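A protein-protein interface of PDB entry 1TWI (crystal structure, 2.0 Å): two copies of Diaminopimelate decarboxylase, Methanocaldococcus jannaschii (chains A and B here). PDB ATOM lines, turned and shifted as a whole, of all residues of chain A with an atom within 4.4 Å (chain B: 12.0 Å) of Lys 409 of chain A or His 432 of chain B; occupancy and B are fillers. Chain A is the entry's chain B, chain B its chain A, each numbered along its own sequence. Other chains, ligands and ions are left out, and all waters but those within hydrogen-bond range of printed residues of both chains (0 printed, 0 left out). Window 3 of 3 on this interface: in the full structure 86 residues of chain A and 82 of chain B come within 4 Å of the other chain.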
ATOM      1  N   GLU A  37     -21.540  20.305 -26.879  1.00  0.00           N
ATOM      2  CA  GLU A  37     -21.737  20.784 -25.507  1.00  0.00           C
ATOM      3  C   GLU A  37     -22.902  20.072 -24.813  1.00  0.00           C
ATOM      4  O   GLU A  37     -22.836  19.685 -23.623  1.00  0.00           O
ATOM      5  CB  GLU A  37     -21.995  22.308 -25.531  1.00  0.00           C
ATOM      6  CG  GLU A  37     -22.331  22.904 -24.187  1.00  0.00           C
ATOM      7  CD  GLU A  37     -22.354  24.427 -24.307  1.00  0.00           C
ATOM      8  OE1 GLU A  37     -21.317  25.075 -24.018  1.00  0.00           O
ATOM      9  OE2 GLU A  37     -23.395  24.989 -24.743  1.00  0.00           O
ATOM     10  N   LYS A  82     -18.224  24.826 -14.942  1.00  0.00           N
ATOM     11  CA  LYS A  82     -19.468  25.564 -14.793  1.00  0.00           C
ATOM     12  C   LYS A  82     -20.623  24.609 -14.442  1.00  0.00           C
ATOM     13  O   LYS A  82     -21.578  25.014 -13.778  1.00  0.00           O
ATOM     14  CB  LYS A  82     -19.776  26.377 -16.057  1.00  0.00           C
ATOM     15  CG  LYS A  82     -18.997  27.720 -16.100  1.00  0.00           C
ATOM     16  CD  LYS A  82     -19.207  28.469 -17.422  1.00  0.00           C
ATOM     17  CE  LYS A  82     -18.698  29.939 -17.378  1.00  0.00           C
ATOM     18  NZ  LYS A  82     -17.599  30.125 -16.370  1.00  0.00           N
ATOM     19  N   SER A 407     -23.039  24.330 -29.798  1.00  0.00           N
ATOM     20  CA  SER A 407     -23.790  24.697 -28.593  1.00  0.00           C
ATOM     21  C   SER A 407     -25.114  25.388 -28.986  1.00  0.00           C
ATOM     22  O   SER A 407     -25.252  25.824 -30.115  1.00  0.00           O
ATOM     23  CB  SER A 407     -22.892  25.678 -27.822  1.00  0.00           C
ATOM     24  OG  SER A 407     -23.578  26.515 -26.907  1.00  0.00           O
ATOM     25  N   LYS A 408     -26.038  25.532 -28.051  1.00  0.00           N
ATOM     26  CA  LYS A 408     -27.307  26.245 -28.328  1.00  0.00           C
ATOM     27  C   LYS A 408     -26.937  27.690 -28.616  1.00  0.00           C
ATOM     28  O   LYS A 408     -27.675  28.401 -29.275  1.00  0.00           O
ATOM     29  CB  LYS A 408     -28.241  26.204 -27.100  1.00  0.00           C
ATOM     30  CG  LYS A 408     -28.820  24.814 -26.866  1.00  0.00           C
ATOM     31  CD  LYS A 408     -29.818  24.756 -25.712  1.00  0.00           C
ATOM     32  CE  LYS A 408     -30.288  23.308 -25.514  1.00  0.00           C
ATOM     33  NZ  LYS A 408     -31.303  23.180 -24.417  1.00  0.00           N
ATOM     34  N   LYS A 409     -25.776  28.124 -28.134  1.00  0.00           N
ATOM     35  CA  LYS A 409     -25.327  29.511 -28.365  1.00  0.00           C
ATOM     36  C   LYS A 409     -24.624  29.732 -29.695  1.00  0.00           C
ATOM     37  O   LYS A 409     -24.348  30.864 -30.058  1.00  0.00           O
ATOM     38  CB  LYS A 409     -24.389  29.950 -27.263  1.00  0.00           C
ATOM     39  CG  LYS A 409     -25.014  29.970 -25.919  1.00  0.00           C
ATOM     40  CD  LYS A 409     -25.486  31.337 -25.588  1.00  0.00           C
ATOM     41  CE  LYS A 409     -25.515  31.494 -24.075  1.00  0.00           C
ATOM     42  NZ  LYS A 409     -25.857  32.899 -23.752  1.00  0.00           N
ATOM     43  N   GLY A 410     -24.345  28.667 -30.441  1.00  0.00           N
ATOM     44  CA  GLY A 410     -23.636  28.858 -31.715  1.00  0.00           C
ATOM     45  C   GLY A 410     -22.488  27.827 -31.834  1.00  0.00           C
ATOM     46  O   GLY A 410     -22.380  26.941 -30.993  1.00  0.00           O
ATOM     47  N   PHE A 412     -18.452  27.316 -31.832  1.00  0.00           N
ATOM     48  CA  PHE A 412     -17.278  28.111 -31.474  1.00  0.00           C
ATOM     49  C   PHE A 412     -15.958  27.414 -31.708  1.00  0.00           C
ATOM     50  O   PHE A 412     -15.827  26.221 -31.371  1.00  0.00           O
ATOM     51  CB  PHE A 412     -17.369  28.459 -29.977  1.00  0.00           C
ATOM     52  CG  PHE A 412     -18.632  29.209 -29.614  1.00  0.00           C
ATOM     53  CD1 PHE A 412     -19.788  28.538 -29.223  1.00  0.00           C
ATOM     54  CD2 PHE A 412     -18.661  30.597 -29.734  1.00  0.00           C
ATOM     55  CE1 PHE A 412     -20.986  29.250 -28.944  1.00  0.00           C
ATOM     56  CE2 PHE A 412     -19.828  31.328 -29.475  1.00  0.00           C
ATOM     57  CZ  PHE A 412     -20.992  30.653 -29.078  1.00  0.00           C
ATOM     58  N   ILE B 428      -9.185  28.193 -26.985  1.00  0.00           N
ATOM     59  CA  ILE B 428      -9.931  29.465 -26.904  1.00  0.00           C
ATOM     60  C   ILE B 428     -11.275  29.234 -26.215  1.00  0.00           C
ATOM     61  O   ILE B 428     -12.084  28.447 -26.686  1.00  0.00           O
ATOM     62  CB  ILE B 428     -10.239  30.017 -28.303  1.00  0.00           C
ATOM     63  CG1 ILE B 428      -8.913  30.337 -29.032  1.00  0.00           C
ATOM     64  CG2 ILE B 428     -11.121  31.274 -28.192  1.00  0.00           C
ATOM     65  CD1 ILE B 428      -8.475  29.200 -29.891  1.00  0.00           C
ATOM     66  N   VAL B 429     -11.503  29.931 -25.117  1.00  0.00           N
ATOM     67  CA  VAL B 429     -12.758  29.817 -24.358  1.00  0.00           C
ATOM     68  C   VAL B 429     -13.820  30.740 -24.956  1.00  0.00           C
ATOM     69  O   VAL B 429     -13.579  31.941 -25.103  1.00  0.00           O
ATOM     70  CB  VAL B 429     -12.531  30.218 -22.903  1.00  0.00           C
ATOM     71  CG1 VAL B 429     -13.892  30.106 -22.111  1.00  0.00           C
ATOM     72  CG2 VAL B 429     -11.408  29.327 -22.283  1.00  0.00           C
ATOM     73  N   PRO B 430     -14.999  30.200 -25.293  1.00  0.00           N
ATOM     74  CA  PRO B 430     -16.108  30.993 -25.883  1.00  0.00           C
ATOM     75  C   PRO B 430     -16.641  31.907 -24.819  1.00  0.00           C
ATOM     76  O   PRO B 430     -16.519  31.611 -23.639  1.00  0.00           O
ATOM     77  CB  PRO B 430     -17.166  29.944 -26.279  1.00  0.00           C
ATOM     78  CG  PRO B 430     -16.464  28.615 -26.109  1.00  0.00           C
ATOM     79  CD  PRO B 430     -15.407  28.791 -25.076  1.00  0.00           C
ATOM     80  N   PRO B 431     -17.278  33.009 -25.222  1.00  0.00           N
ATOM     81  CA  PRO B 431     -17.825  34.006 -24.285  1.00  0.00           C
ATOM     82  C   PRO B 431     -18.709  33.436 -23.188  1.00  0.00           C
ATOM     83  O   PRO B 431     -18.555  33.801 -22.026  1.00  0.00           O
ATOM     84  CB  PRO B 431     -18.591  34.985 -25.221  1.00  0.00           C
ATOM     85  CG  PRO B 431     -17.772  34.944 -26.474  1.00  0.00           C
ATOM     86  CD  PRO B 431     -17.461  33.439 -26.625  1.00  0.00           C
ATOM     87  N   HIS B 432     -19.596  32.510 -23.525  1.00  0.00           N
ATOM     88  CA  HIS B 432     -20.491  31.976 -22.477  1.00  0.00           C
ATOM     89  C   HIS B 432     -19.820  31.060 -21.477  1.00  0.00           C
ATOM     90  O   HIS B 432     -20.415  30.685 -20.462  1.00  0.00           O
ATOM     91  CB  HIS B 432     -21.763  31.286 -23.082  1.00  0.00           C
ATOM     92  CG  HIS B 432     -21.484  29.963 -23.747  1.00  0.00           C
ATOM     93  ND1 HIS B 432     -21.015  29.866 -25.037  1.00  0.00           N
ATOM     94  CD2 HIS B 432     -21.592  28.690 -23.291  1.00  0.00           C
ATOM     95  CE1 HIS B 432     -20.844  28.593 -25.353  1.00  0.00           C
ATOM     96  NE2 HIS B 432     -21.191  27.857 -24.308  1.00  0.00           N
ATOM     97  N   LEU B 433     -18.558  30.727 -21.728  1.00  0.00           N
ATOM     98  CA  LEU B 433     -17.806  29.852 -20.827  1.00  0.00           C
ATOM     99  C   LEU B 433     -16.715  30.641 -20.061  1.00  0.00           C
ATOM    100  O   LEU B 433     -15.956  30.060 -19.297  1.00  0.00           O
ATOM    101  CB  LEU B 433     -17.141  28.676 -21.614  1.00  0.00           C
ATOM    102  CG  LEU B 433     -18.119  27.697 -22.303  1.00  0.00           C
ATOM    103  CD1 LEU B 433     -17.378  26.496 -22.913  1.00  0.00           C
ATOM    104  CD2 LEU B 433     -19.156  27.174 -21.268  1.00  0.00           C
ATOM    105  N   LEU B 434     -16.640  31.955 -20.261  1.00  0.00           N
ATOM    106  CA  LEU B 434     -15.631  32.763 -19.532  1.00  0.00           C
ATOM    107  C   LEU B 434     -16.054  32.922 -18.089  1.00  0.00           C
ATOM    108  O   LEU B 434     -17.278  32.874 -17.864  1.00  0.00           O
ATOM    109  CB  LEU B 434     -15.525  34.163 -20.128  1.00  0.00           C
ATOM    110  CG  LEU B 434     -14.731  34.133 -21.425  1.00  0.00           C
ATOM    111  CD1 LEU B 434     -14.862  35.440 -22.139  1.00  0.00           C
ATOM    112  CD2 LEU B 434     -13.270  33.815 -21.079  1.00  0.00           C
ATOM    113  OXT LEU B 434     -15.166  33.144 -17.217  1.00  0.00           O
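Of the printed residues of chain B, Glu 37 of chain A touches His 432 (2.8 Å).
Ser 407 of chain A touches just one residue of chain B: His 432.
Of chain B, only His 432 comes within 4 Å of Lys 409 of chain A.
Printed residues of chain B within 4 Å of Phe 412 of chain A: Pro 430 (3.7 Å) and His 432 (3.7 Å).
Ile 428 of chain B touches none of the printed residues of chain A.
Of chain A, only Glu 37 (2.8 Å), Lys 82 (3.6 Å), Ser 407 (3.8 Å), Lys 409 (3.9 Å) and Phe 412 (3.7 Å) come within 4 Å of His 432 of chain B.
Of the printed residues of chain A, Leu 433 of chain B touches Lys 82 (3.3 Å).
Printed residues of chain A within 4 Å of Leu 434 of chain B: Lys 82 (3.1 Å).
The nearest residue of chain B that does not touch Lys 409 of chain A is Pro 431 of chain B (7.1 Å).
The nearest printed residue of chain A that does not touch His 432 of chain B is Gly 410 of chain A (6.1 Å).
The nearest printed residue of chain A that does not touch Pro 430 of chain B is Glu 37 of chain A (6.4 Å).
A ring nitrogen (NE2) of His 432 of chain B is in hydrogen-bond range of the side-chain carboxylate (OE1) of Glu 37 of chain A (2.8 Å).
The side-chain amino group (NZ) of Lys 82 of chain A sits close to the backbone carbonyl oxygen (O) of Leu 433 of chain B.
O of Leu 434 of chain B is in salt-bridge range of NZ of Lys 82 of chain A (3.1 Å).
No position is printed for both chains.
Of the 8 pairs that touch across the chains among the printed residues, none has its exchanged pair printed and touching as well.
Hydrophobic or aromatic side chains of chain A that line the printed part of chain B: Phe 412.
Along chain A the printed residues that touch a printed residue of chain B span positions 37 to 412.
Among the printed residues, no Asp or Glu carboxylate lies within 4 Å of a Lys or Arg side-chain nitrogen of the other chain.
Among the printed residues, pairs that only touch across the chains: Lys 82 of chain A with His 432 of chain B (3.6 Å), Phe 412 of chain A with His 432 of chain B (3.7 Å), Phe 412 of chain A with Pro 430 of chain B (3.7 Å), Ser 407 of chain A with His 432 of chain B (3.8 Å) and Lys 409 of chain A with His 432 of chain B (3.9 Å).
The side-chain carboxylate (OE2) of Glu 37 of chain A lies within hydrogen-bond range of the side-chain hydroxyl (OG) of Ser 407 of chain A.
OG of Ser 407 of chain A lies close to N of Lys 409 of chain A (3.0 Å).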
